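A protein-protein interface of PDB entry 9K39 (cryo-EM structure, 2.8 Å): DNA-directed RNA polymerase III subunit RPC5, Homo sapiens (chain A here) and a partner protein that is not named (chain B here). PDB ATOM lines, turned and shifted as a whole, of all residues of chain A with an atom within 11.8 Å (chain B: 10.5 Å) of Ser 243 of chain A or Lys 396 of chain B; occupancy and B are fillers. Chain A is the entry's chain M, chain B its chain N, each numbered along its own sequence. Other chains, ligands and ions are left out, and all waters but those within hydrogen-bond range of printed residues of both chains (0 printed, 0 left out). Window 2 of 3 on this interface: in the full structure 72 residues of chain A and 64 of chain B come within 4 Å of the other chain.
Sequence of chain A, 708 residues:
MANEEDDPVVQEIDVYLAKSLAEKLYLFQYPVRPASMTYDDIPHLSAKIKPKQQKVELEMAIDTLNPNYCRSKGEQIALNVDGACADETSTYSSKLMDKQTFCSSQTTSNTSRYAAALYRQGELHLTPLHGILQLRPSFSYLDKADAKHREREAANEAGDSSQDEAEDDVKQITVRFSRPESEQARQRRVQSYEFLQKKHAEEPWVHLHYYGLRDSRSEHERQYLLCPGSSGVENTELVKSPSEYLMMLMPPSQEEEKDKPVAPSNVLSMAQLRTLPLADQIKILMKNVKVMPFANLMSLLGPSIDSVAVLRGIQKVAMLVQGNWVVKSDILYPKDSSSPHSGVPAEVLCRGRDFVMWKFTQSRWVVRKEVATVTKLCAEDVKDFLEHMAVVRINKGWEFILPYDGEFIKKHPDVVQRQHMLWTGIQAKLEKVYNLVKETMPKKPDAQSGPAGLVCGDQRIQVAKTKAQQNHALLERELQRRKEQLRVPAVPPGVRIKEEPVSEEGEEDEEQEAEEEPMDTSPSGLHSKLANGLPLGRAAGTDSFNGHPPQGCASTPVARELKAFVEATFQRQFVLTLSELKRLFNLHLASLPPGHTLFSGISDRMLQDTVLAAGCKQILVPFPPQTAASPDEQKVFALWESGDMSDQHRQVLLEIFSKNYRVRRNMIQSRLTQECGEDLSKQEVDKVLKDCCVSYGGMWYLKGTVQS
The backbone carbonyl oxygen (O) of Val 239 of chain A is in hydrogen-bond range of the side-chain amino group (NZ) of Lys 343 of chain B. OH of Tyr 245 of chain A lies within hydrogen-bond range of O of Thr 274 of chain B (2.5 Å).
The backbone NH of Glu 244 of chain A sits close to the side-chain hydroxyl of Ser 241 of chain A, 3.4 Å away.
Among the printed residues, merely in contact across the chains: Leu 238 of chain A with Pro 276 of chain B, Met 248 of chain A with Gly 277 of chain B, Tyr 245 of chain A with Pro 276 of chain B, Leu 249 of chain A with Phe 389 of chain B, Lys 240 of chain A with Lys 343 of chain B, Leu 249 of chain A with Thr 274 of chain B, Pro 242 of chain A with Leu 392 of chain B, Pro 242 of chain A with Val 344 of chain B, Leu 238 of chain A with Gly 277 of chain B, Ser 243 of chain A with Lys 396 of chain B, Tyr 245 of chain A with Val 344 of chain B, Ser 241 of chain A with Lys 343 of chain B, Leu 246 of chain A with Leu 393 of chain B, Val 239 of chain A with Pro 276 of chain B and Lys 240 of chain A with Pro 276 of chain B.
Ser 243 of chain A touches one residue of chain B. Lys 396 of chain B touches just one residue of chain A: Ser 243 (3.7 Å). Pro 242 of chain A touches just these residues of chain B: Val 344 and Leu 392. Of the printed residues of chain B, Leu 246 of chain A touches Leu 393. No residue of chain B comes within 4 Å of Met 247 of chain A. No residue of chain A comes within 4 Å of Asp 394 of chain B. No residue of chain A comes within 4 Å of His 395 of chain B. Of the printed residues of chain B, Val 239 of chain A touches Pro 276 and Lys 343. Printed residues of chain A within 4 Å of Thr 274 of chain B: Tyr 245 (2.5 Å) and Leu 249 (3.6 Å). Of the printed residues of chain A, Pro 276 of chain B touches Leu 238, Val 239, Lys 240 and Tyr 245. Arg 274 of chain A touches none of the printed residues of chain B. Pro 251 of chain A touches none of the printed residues of chain B. The nearest residue of chain B that does not touch Ser 243 of chain A is His 395 of chain B (5.0 Å). The nearest residue of chain A that does not touch Lys 396 of chain B is Ser 241 of chain A (4.9 Å). The nearest printed residue of chain B that does not touch Lys 240 of chain A is Gly 277 of chain B (4.3 Å).
Hydrophobic or aromatic side chains of chain A that line the printed part of chain B: Leu 238, Val 239, Pro 242, Tyr 245, Leu 246, Met 248 and Leu 249. Among the printed residues, 17 pairs touch across the chains. Among the printed residues, no Asp or Glu carboxylate lies within 4 Å of a Lys or Arg side-chain nitrogen of the other chain.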
ATOM      1  N   LEU A 238     -18.573 -21.448  13.194  1.00  0.00           N
ATOM      2  CA  LEU A 238     -17.138 -21.505  13.480  1.00  0.00           C
ATOM      3  C   LEU A 238     -16.814 -22.670  14.416  1.00  0.00           C
ATOM      4  O   LEU A 238     -16.052 -22.536  15.377  1.00  0.00           O
ATOM      5  CB  LEU A 238     -16.632 -20.178  14.054  1.00  0.00           C
ATOM      6  CG  LEU A 238     -16.827 -18.929  13.190  1.00  0.00           C
ATOM      7  CD1 LEU A 238     -16.322 -17.692  13.916  1.00  0.00           C
ATOM      8  CD2 LEU A 238     -16.129 -19.088  11.849  1.00  0.00           C
ATOM      9  N   VAL A 239     -17.407 -23.827  14.124  1.00  0.00           N
ATOM     10  CA  VAL A 239     -17.254 -25.025  14.939  1.00  0.00           C
ATOM     11  C   VAL A 239     -16.732 -26.207  14.133  1.00  0.00           C
ATOM     12  O   VAL A 239     -16.808 -27.345  14.593  1.00  0.00           O
ATOM     13  CB  VAL A 239     -18.577 -25.391  15.642  1.00  0.00           C
ATOM     14  CG1 VAL A 239     -18.976 -24.303  16.626  1.00  0.00           C
ATOM     15  CG2 VAL A 239     -19.675 -25.619  14.615  1.00  0.00           C
ATOM     16  N   LYS A 240     -16.206 -25.965  12.936  1.00  0.00           N
ATOM     17  CA  LYS A 240     -15.696 -27.055  12.117  1.00  0.00           C
ATOM     18  C   LYS A 240     -14.329 -27.511  12.613  1.00  0.00           C
ATOM     19  O   LYS A 240     -13.542 -26.719  13.139  1.00  0.00           O
ATOM     20  CB  LYS A 240     -15.613 -26.632  10.651  1.00  0.00           C
ATOM     21  CG  LYS A 240     -16.968 -26.498   9.975  1.00  0.00           C
ATOM     22  CD  LYS A 240     -16.839 -26.482   8.462  1.00  0.00           C
ATOM     23  CE  LYS A 240     -18.205 -26.528   7.798  1.00  0.00           C
ATOM     24  NZ  LYS A 240     -18.107 -26.652   6.317  1.00  0.00           N
ATOM     25  N   SER A 241     -14.051 -28.802  12.442  1.00  0.00           N
ATOM     26  CA  SER A 241     -12.797 -29.379  12.887  1.00  0.00           C
ATOM     27  C   SER A 241     -11.641 -28.889  12.016  1.00  0.00           C
ATOM     28  O   SER A 241     -11.853 -28.392  10.907  1.00  0.00           O
ATOM     29  CB  SER A 241     -12.877 -30.903  12.853  1.00  0.00           C
ATOM     30  OG  SER A 241     -13.065 -31.375  11.530  1.00  0.00           O
ATOM     31  N   PRO A 242     -10.400 -29.005  12.508  1.00  0.00           N
ATOM     32  CA  PRO A 242      -9.247 -28.623  11.675  1.00  0.00           C
ATOM     33  C   PRO A 242      -9.191 -29.349  10.343  1.00  0.00           C
ATOM     34  O   PRO A 242      -8.799 -28.752   9.332  1.00  0.00           O
ATOM     35  CB  PRO A 242      -8.050 -28.971  12.566  1.00  0.00           C
ATOM     36  CG  PRO A 242      -8.574 -28.837  13.952  1.00  0.00           C
ATOM     37  CD  PRO A 242      -9.998 -29.316  13.893  1.00  0.00           C
ATOM     38  N   SER A 243      -9.568 -30.630  10.309  1.00  0.00           N
ATOM     39  CA  SER A 243      -9.574 -31.364   9.048  1.00  0.00           C
ATOM     40  C   SER A 243     -10.592 -30.780   8.076  1.00  0.00           C
ATOM     41  O   SER A 243     -10.305 -30.623   6.884  1.00  0.00           O
ATOM     42  CB  SER A 243      -9.859 -32.844   9.303  1.00  0.00           C
ATOM     43  OG  SER A 243      -9.857 -33.580   8.092  1.00  0.00           O
ATOM     44  N   GLU A 244     -11.788 -30.451   8.570  1.00  0.00           N
ATOM     45  CA  GLU A 244     -12.799 -29.839   7.714  1.00  0.00           C
ATOM     46  C   GLU A 244     -12.338 -28.477   7.208  1.00  0.00           C
ATOM     47  O   GLU A 244     -12.559 -28.136   6.040  1.00  0.00           O
ATOM     48  CB  GLU A 244     -14.124 -29.715   8.469  1.00  0.00           C
ATOM     49  CG  GLU A 244     -14.772 -31.048   8.802  1.00  0.00           C
ATOM     50  CD  GLU A 244     -16.045 -30.892   9.611  1.00  0.00           C
ATOM     51  OE1 GLU A 244     -16.370 -29.750   9.997  1.00  0.00           O
ATOM     52  OE2 GLU A 244     -16.722 -31.913   9.861  1.00  0.00           O
ATOM     53  N   TYR A 245     -11.689 -27.690   8.068  1.00  0.00           N
ATOM     54  CA  TYR A 245     -11.171 -26.395   7.637  1.00  0.00           C
ATOM     55  C   TYR A 245     -10.109 -26.564   6.555  1.00  0.00           C
ATOM     56  O   TYR A 245     -10.106 -25.827   5.559  1.00  0.00           O
ATOM     57  CB  TYR A 245     -10.600 -25.631   8.830  1.00  0.00           C
ATOM     58  CG  TYR A 245     -10.282 -24.180   8.544  1.00  0.00           C
ATOM     59  CD1 TYR A 245     -10.907 -23.505   7.503  1.00  0.00           C
ATOM     60  CD2 TYR A 245      -9.349 -23.489   9.305  1.00  0.00           C
ATOM     61  CE1 TYR A 245     -10.620 -22.180   7.236  1.00  0.00           C
ATOM     62  CE2 TYR A 245      -9.053 -22.166   9.045  1.00  0.00           C
ATOM     63  CZ  TYR A 245      -9.690 -21.516   8.008  1.00  0.00           C
ATOM     64  OH  TYR A 245      -9.399 -20.197   7.744  1.00  0.00           O
ATOM     65  N   LEU A 246      -9.201 -27.524   6.734  1.00  0.00           N
ATOM     66  CA  LEU A 246      -8.159 -27.757   5.738  1.00  0.00           C
ATOM     67  C   LEU A 246      -8.756 -28.224   4.418  1.00  0.00           C
ATOM     68  O   LEU A 246      -8.287 -27.833   3.342  1.00  0.00           O
ATOM     69  CB  LEU A 246      -7.149 -28.776   6.265  1.00  0.00           C
ATOM     70  CG  LEU A 246      -5.952 -29.088   5.363  1.00  0.00           C
ATOM     71  CD1 LEU A 246      -5.173 -27.823   5.046  1.00  0.00           C
ATOM     72  CD2 LEU A 246      -5.053 -30.124   6.014  1.00  0.00           C
ATOM     73  N   MET A 247      -9.790 -29.068   4.475  1.00  0.00           N
ATOM     74  CA  MET A 247     -10.464 -29.489   3.250  1.00  0.00           C
ATOM     75  C   MET A 247     -11.173 -28.315   2.583  1.00  0.00           C
ATOM     76  O   MET A 247     -11.257 -28.251   1.350  1.00  0.00           O
ATOM     77  CB  MET A 247     -11.454 -30.614   3.551  1.00  0.00           C
ATOM     78  CG  MET A 247     -10.814 -31.916   4.019  1.00  0.00           C
ATOM     79  SD  MET A 247      -9.675 -32.636   2.819  1.00  0.00           S
ATOM     80  CE  MET A 247      -8.095 -32.209   3.545  1.00  0.00           C
ATOM     81  N   MET A 248     -11.691 -27.381   3.381  1.00  0.00           N
ATOM     82  CA  MET A 248     -12.375 -26.221   2.818  1.00  0.00           C
ATOM     83  C   MET A 248     -11.395 -25.287   2.116  1.00  0.00           C
ATOM     84  O   MET A 248     -11.600 -24.920   0.954  1.00  0.00           O
ATOM     85  CB  MET A 248     -13.134 -25.476   3.917  1.00  0.00           C
ATOM     86  CG  MET A 248     -13.792 -24.188   3.444  1.00  0.00           C
ATOM     87  SD  MET A 248     -14.577 -23.269   4.782  1.00  0.00           S
ATOM     88  CE  MET A 248     -15.788 -24.462   5.344  1.00  0.00           C
ATOM     89  N   LEU A 249     -10.326 -24.890   2.808  1.00  0.00           N
ATOM     90  CA  LEU A 249      -9.374 -23.948   2.227  1.00  0.00           C
ATOM     91  C   LEU A 249      -8.455 -24.587   1.196  1.00  0.00           C
ATOM     92  O   LEU A 249      -7.700 -23.865   0.533  1.00  0.00           O
ATOM     93  CB  LEU A 249      -8.545 -23.280   3.333  1.00  0.00           C
ATOM     94  CG  LEU A 249      -7.763 -24.139   4.334  1.00  0.00           C
ATOM     95  CD1 LEU A 249      -6.377 -24.490   3.820  1.00  0.00           C
ATOM     96  CD2 LEU A 249      -7.673 -23.439   5.682  1.00  0.00           C
ATOM     97  N   MET A 250      -8.496 -25.909   1.042  1.00  0.00           N
ATOM     98  CA  MET A 250      -7.749 -26.619   0.003  1.00  0.00           C
ATOM     99  C   MET A 250      -8.677 -27.627  -0.665  1.00  0.00           C
ATOM    100  O   MET A 250      -8.602 -28.833  -0.403  1.00  0.00           O
ATOM    101  CB  MET A 250      -6.513 -27.311   0.578  1.00  0.00           C
ATOM    102  CG  MET A 250      -5.384 -26.365   0.947  1.00  0.00           C
ATOM    103  SD  MET A 250      -4.816 -25.381  -0.452  1.00  0.00           S
ATOM    104  CE  MET A 250      -4.262 -26.669  -1.570  1.00  0.00           C
ATOM    105  N   PRO A 251      -9.574 -27.159  -1.537  1.00  0.00           N
ATOM    106  CA  PRO A 251     -10.491 -28.083  -2.197  1.00  0.00           C
ATOM    107  C   PRO A 251      -9.758 -28.928  -3.225  1.00  0.00           C
ATOM    108  O   PRO A 251      -8.780 -28.470  -3.842  1.00  0.00           O
ATOM    109  CB  PRO A 251     -11.513 -27.148  -2.867  1.00  0.00           C
ATOM    110  CG  PRO A 251     -10.749 -25.896  -3.114  1.00  0.00           C
ATOM    111  CD  PRO A 251      -9.792 -25.763  -1.957  1.00  0.00           C
ATOM    112  N   PRO A 252     -10.190 -30.167  -3.440  1.00  0.00           N
ATOM    113  CA  PRO A 252      -9.536 -31.012  -4.444  1.00  0.00           C
ATOM    114  C   PRO A 252      -9.749 -30.478  -5.853  1.00  0.00           C
ATOM    115  O   PRO A 252     -10.686 -29.720  -6.122  1.00  0.00           O
ATOM    116  CB  PRO A 252     -10.212 -32.376  -4.262  1.00  0.00           C
ATOM    117  CG  PRO A 252     -10.823 -32.330  -2.894  1.00  0.00           C
ATOM    118  CD  PRO A 252     -11.218 -30.902  -2.684  1.00  0.00           C
ATOM    119  N   ARG A 274      -5.023 -48.301   0.251  1.00  0.00           N
ATOM    120  CA  ARG A 274      -5.920 -48.190   1.395  1.00  0.00           C
ATOM    121  C   ARG A 274      -7.286 -47.632   1.015  1.00  0.00           C
ATOM    122  O   ARG A 274      -8.262 -47.880   1.731  1.00  0.00           O
ATOM    123  CB  ARG A 274      -5.284 -47.316   2.478  1.00  0.00           C
ATOM    124  CG  ARG A 274      -4.017 -47.901   3.082  1.00  0.00           C
ATOM    125  CD  ARG A 274      -3.419 -46.974   4.132  1.00  0.00           C
ATOM    126  NE  ARG A 274      -2.194 -47.517   4.714  1.00  0.00           N
ATOM    127  CZ  ARG A 274      -1.475 -46.902   5.647  1.00  0.00           C
ATOM    128  NH1 ARG A 274      -1.856 -45.719   6.109  1.00  0.00           N
ATOM    129  NH2 ARG A 274      -0.374 -47.470   6.120  1.00  0.00           N
ATOM    130  N   THR B 274     -11.190 -17.939   3.534  1.00  0.00           N
ATOM    131  CA  THR B 274     -12.265 -18.735   4.113  1.00  0.00           C
ATOM    132  C   THR B 274     -12.034 -18.882   5.612  1.00  0.00           C
ATOM    133  O   THR B 274     -10.942 -19.270   6.040  1.00  0.00           O
ATOM    134  CB  THR B 274     -12.347 -20.117   3.458  1.00  0.00           C
ATOM    135  OG1 THR B 274     -11.118 -20.822   3.668  1.00  0.00           O
ATOM    136  CG2 THR B 274     -12.599 -19.984   1.962  1.00  0.00           C
ATOM    137  N   PRO B 276     -12.930 -20.689   9.347  1.00  0.00           N
ATOM    138  CA  PRO B 276     -13.295 -22.059   9.738  1.00  0.00           C
ATOM    139  C   PRO B 276     -14.730 -22.179  10.220  1.00  0.00           C
ATOM    140  O   PRO B 276     -14.972 -22.540  11.376  1.00  0.00           O
ATOM    141  CB  PRO B 276     -12.302 -22.371  10.864  1.00  0.00           C
ATOM    142  CG  PRO B 276     -11.981 -21.039  11.446  1.00  0.00           C
ATOM    143  CD  PRO B 276     -11.962 -20.088  10.283  1.00  0.00           C
ATOM    144  N   GLY B 277     -15.691 -21.888   9.345  1.00  0.00           N
ATOM    145  CA  GLY B 277     -17.091 -21.966   9.699  1.00  0.00           C
ATOM    146  C   GLY B 277     -17.947 -22.217   8.477  1.00  0.00           C
ATOM    147  O   GLY B 277     -17.449 -22.366   7.360  1.00  0.00           O
ATOM    148  N   GLU B 313     -19.424 -26.021   0.572  1.00  0.00           N
ATOM    149  CA  GLU B 313     -18.054 -25.726   0.999  1.00  0.00           C
ATOM    150  C   GLU B 313     -17.538 -24.442   0.350  1.00  0.00           C
ATOM    151  O   GLU B 313     -16.381 -24.355  -0.069  1.00  0.00           O
ATOM    152  CB  GLU B 313     -17.115 -26.899   0.712  1.00  0.00           C
ATOM    153  CG  GLU B 313     -17.456 -28.178   1.466  1.00  0.00           C
ATOM    154  CD  GLU B 313     -18.509 -29.013   0.764  1.00  0.00           C
ATOM    155  OE1 GLU B 313     -18.572 -28.969  -0.483  1.00  0.00           O
ATOM    156  OE2 GLU B 313     -19.275 -29.714   1.458  1.00  0.00           O
ATOM    157  N   LYS B 343     -12.421 -24.313  16.873  1.00  0.00           N
ATOM    158  CA  LYS B 343     -11.584 -25.491  17.085  1.00  0.00           C
ATOM    159  C   LYS B 343     -10.161 -25.270  16.587  1.00  0.00           C
ATOM    160  O   LYS B 343      -9.222 -25.877  17.115  1.00  0.00           O
ATOM    161  CB  LYS B 343     -12.208 -26.708  16.405  1.00  0.00           C
ATOM    162  CG  LYS B 343     -13.529 -27.143  17.016  1.00  0.00           C
ATOM    163  CD  LYS B 343     -14.055 -28.406  16.357  1.00  0.00           C
ATOM    164  CE  LYS B 343     -15.333 -28.885  17.028  1.00  0.00           C
ATOM    165  NZ  LYS B 343     -16.415 -27.864  16.961  1.00  0.00           N
ATOM    166  N   VAL B 344      -9.978 -24.417  15.583  1.00  0.00           N
ATOM    167  CA  VAL B 344      -8.663 -24.143  15.031  1.00  0.00           C
ATOM    168  C   VAL B 344      -8.133 -22.849  15.629  1.00  0.00           C
ATOM    169  O   VAL B 344      -8.867 -22.059  16.227  1.00  0.00           O
ATOM    170  CB  VAL B 344      -8.689 -24.067  13.488  1.00  0.00           C
ATOM    171  CG1 VAL B 344      -9.511 -25.205  12.911  1.00  0.00           C
ATOM    172  CG2 VAL B 344      -9.226 -22.721  13.031  1.00  0.00           C
ATOM    173  N   THR B 345      -6.830 -22.629  15.469  1.00  0.00           N
ATOM    174  CA  THR B 345      -6.164 -21.433  15.968  1.00  0.00           C
ATOM    175  C   THR B 345      -5.265 -20.877  14.877  1.00  0.00           C
ATOM    176  O   THR B 345      -4.342 -21.559  14.422  1.00  0.00           O
ATOM    177  CB  THR B 345      -5.348 -21.736  17.230  1.00  0.00           C
ATOM    178  OG1 THR B 345      -4.464 -22.835  16.979  1.00  0.00           O
ATOM    179  CG2 THR B 345      -6.264 -22.076  18.397  1.00  0.00           C
ATOM    180  N   ASP B 388      -2.602 -21.683  10.892  1.00  0.00           N
ATOM    181  CA  ASP B 388      -1.452 -22.436  11.394  1.00  0.00           C
ATOM    182  C   ASP B 388      -1.443 -23.794  10.699  1.00  0.00           C
ATOM    183  O   ASP B 388      -1.910 -24.808  11.224  1.00  0.00           O
ATOM    184  CB  ASP B 388      -1.515 -22.570  12.909  1.00  0.00           C
ATOM    185  CG  ASP B 388      -0.233 -23.129  13.500  1.00  0.00           C
ATOM    186  OD1 ASP B 388       0.750 -23.293  12.749  1.00  0.00           O
ATOM    187  OD2 ASP B 388      -0.211 -23.405  14.719  1.00  0.00           O
ATOM    188  N   PHE B 389      -0.890 -23.804   9.482  1.00  0.00           N
ATOM    189  CA  PHE B 389      -0.929 -25.006   8.656  1.00  0.00           C
ATOM    190  C   PHE B 389      -0.156 -26.159   9.283  1.00  0.00           C
ATOM    191  O   PHE B 389      -0.522 -27.322   9.090  1.00  0.00           O
ATOM    192  CB  PHE B 389      -0.386 -24.707   7.259  1.00  0.00           C
ATOM    193  CG  PHE B 389      -1.286 -23.834   6.432  1.00  0.00           C
ATOM    194  CD1 PHE B 389      -2.380 -24.373   5.777  1.00  0.00           C
ATOM    195  CD2 PHE B 389      -1.037 -22.478   6.305  1.00  0.00           C
ATOM    196  CE1 PHE B 389      -3.211 -23.576   5.013  1.00  0.00           C
ATOM    197  CE2 PHE B 389      -1.864 -21.676   5.543  1.00  0.00           C
ATOM    198  CZ  PHE B 389      -2.953 -22.225   4.897  1.00  0.00           C
ATOM    199  N   GLU B 390       0.908 -25.861  10.034  1.00  0.00           N
ATOM    200  CA  GLU B 390       1.680 -26.928  10.664  1.00  0.00           C
ATOM    201  C   GLU B 390       0.830 -27.707  11.662  1.00  0.00           C
ATOM    202  O   GLU B 390       0.855 -28.944  11.676  1.00  0.00           O
ATOM    203  CB  GLU B 390       2.916 -26.344  11.351  1.00  0.00           C
ATOM    204  CG  GLU B 390       3.838 -27.391  11.958  1.00  0.00           C
ATOM    205  CD  GLU B 390       5.084 -26.783  12.570  1.00  0.00           C
ATOM    206  OE1 GLU B 390       5.185 -25.539  12.603  1.00  0.00           O
ATOM    207  OE2 GLU B 390       5.965 -27.548  13.016  1.00  0.00           O
ATOM    208  N   SER B 391       0.066 -27.000  12.497  1.00  0.00           N
ATOM    209  CA  SER B 391      -0.807 -27.673  13.456  1.00  0.00           C
ATOM    210  C   SER B 391      -1.929 -28.421  12.749  1.00  0.00           C
ATOM    211  O   SER B 391      -2.285 -29.536  13.146  1.00  0.00           O
ATOM    212  CB  SER B 391      -1.376 -26.661  14.451  1.00  0.00           C
ATOM    213  OG  SER B 391      -2.157 -25.682  13.790  1.00  0.00           O
ATOM    214  N   LEU B 392      -2.499 -27.822  11.698  1.00  0.00           N
ATOM    215  CA  LEU B 392      -3.551 -28.497  10.946  1.00  0.00           C
ATOM    216  C   LEU B 392      -3.038 -29.769  10.284  1.00  0.00           C
ATOM    217  O   LEU B 392      -3.802 -30.721  10.094  1.00  0.00           O
ATOM    218  CB  LEU B 392      -4.135 -27.552   9.893  1.00  0.00           C
ATOM    219  CG  LEU B 392      -4.674 -26.210  10.390  1.00  0.00           C
ATOM    220  CD1 LEU B 392      -5.260 -25.403   9.242  1.00  0.00           C
ATOM    221  CD2 LEU B 392      -5.704 -26.409  11.491  1.00  0.00           C
ATOM    222  N   LEU B 393      -1.752 -29.806   9.931  1.00  0.00           N
ATOM    223  CA  LEU B 393      -1.188 -30.999   9.306  1.00  0.00           C
ATOM    224  C   LEU B 393      -0.834 -32.058  10.344  1.00  0.00           C
ATOM    225  O   LEU B 393      -1.119 -33.245  10.148  1.00  0.00           O
ATOM    226  CB  LEU B 393       0.039 -30.629   8.471  1.00  0.00           C
ATOM    227  CG  LEU B 393      -0.249 -29.883   7.166  1.00  0.00           C
ATOM    228  CD1 LEU B 393       1.036 -29.611   6.399  1.00  0.00           C
ATOM    229  CD2 LEU B 393      -1.234 -30.664   6.306  1.00  0.00           C
ATOM    230  N   ASP B 394      -0.212 -31.656  11.457  1.00  0.00           N
ATOM    231  CA  ASP B 394       0.140 -32.638  12.479  1.00  0.00           C
ATOM    232  C   ASP B 394      -1.078 -33.140  13.244  1.00  0.00           C
ATOM    233  O   ASP B 394      -0.983 -34.169  13.921  1.00  0.00           O
ATOM    234  CB  ASP B 394       1.185 -32.074  13.450  1.00  0.00           C
ATOM    235  CG  ASP B 394       0.721 -30.817  14.171  1.00  0.00           C
ATOM    236  OD1 ASP B 394      -0.373 -30.823  14.773  1.00  0.00           O
ATOM    237  OD2 ASP B 394       1.480 -29.825  14.165  1.00  0.00           O
ATOM    238  N   HIS B 395      -2.211 -32.440  13.156  1.00  0.00           N
ATOM    239  CA  HIS B 395      -3.424 -32.910  13.821  1.00  0.00           C
ATOM    240  C   HIS B 395      -3.946 -34.184  13.168  1.00  0.00           C
ATOM    241  O   HIS B 395      -4.199 -35.187  13.845  1.00  0.00           O
ATOM    242  CB  HIS B 395      -4.488 -31.812  13.800  1.00  0.00           C
ATOM    243  CG  HIS B 395      -5.739 -32.171  14.539  1.00  0.00           C
ATOM    244  ND1 HIS B 395      -6.850 -32.696  13.912  1.00  0.00           N
ATOM    245  CD2 HIS B 395      -6.059 -32.079  15.851  1.00  0.00           C
ATOM    246  CE1 HIS B 395      -7.797 -32.914  14.807  1.00  0.00           C
ATOM    247  NE2 HIS B 395      -7.343 -32.546  15.991  1.00  0.00           N
ATOM    248  N   LYS B 396      -4.116 -34.162  11.849  1.00  0.00           N
ATOM    249  CA  LYS B 396      -4.558 -35.340  11.108  1.00  0.00           C
ATOM    250  C   LYS B 396      -3.760 -35.504   9.821  1.00  0.00           C
ATOM    251  O   LYS B 396      -4.300 -35.363   8.722  1.00  0.00           O
ATOM    252  CB  LYS B 396      -6.054 -35.254  10.792  1.00  0.00           C
ATOM    253  CG  LYS B 396      -6.962 -35.430  11.999  1.00  0.00           C
ATOM    254  CD  LYS B 396      -8.425 -35.421  11.591  1.00  0.00           C
ATOM    255  CE  LYS B 396      -9.337 -35.612  12.794  1.00  0.00           C
ATOM    256  NZ  LYS B 396     -10.773 -35.627  12.407  1.00  0.00           N
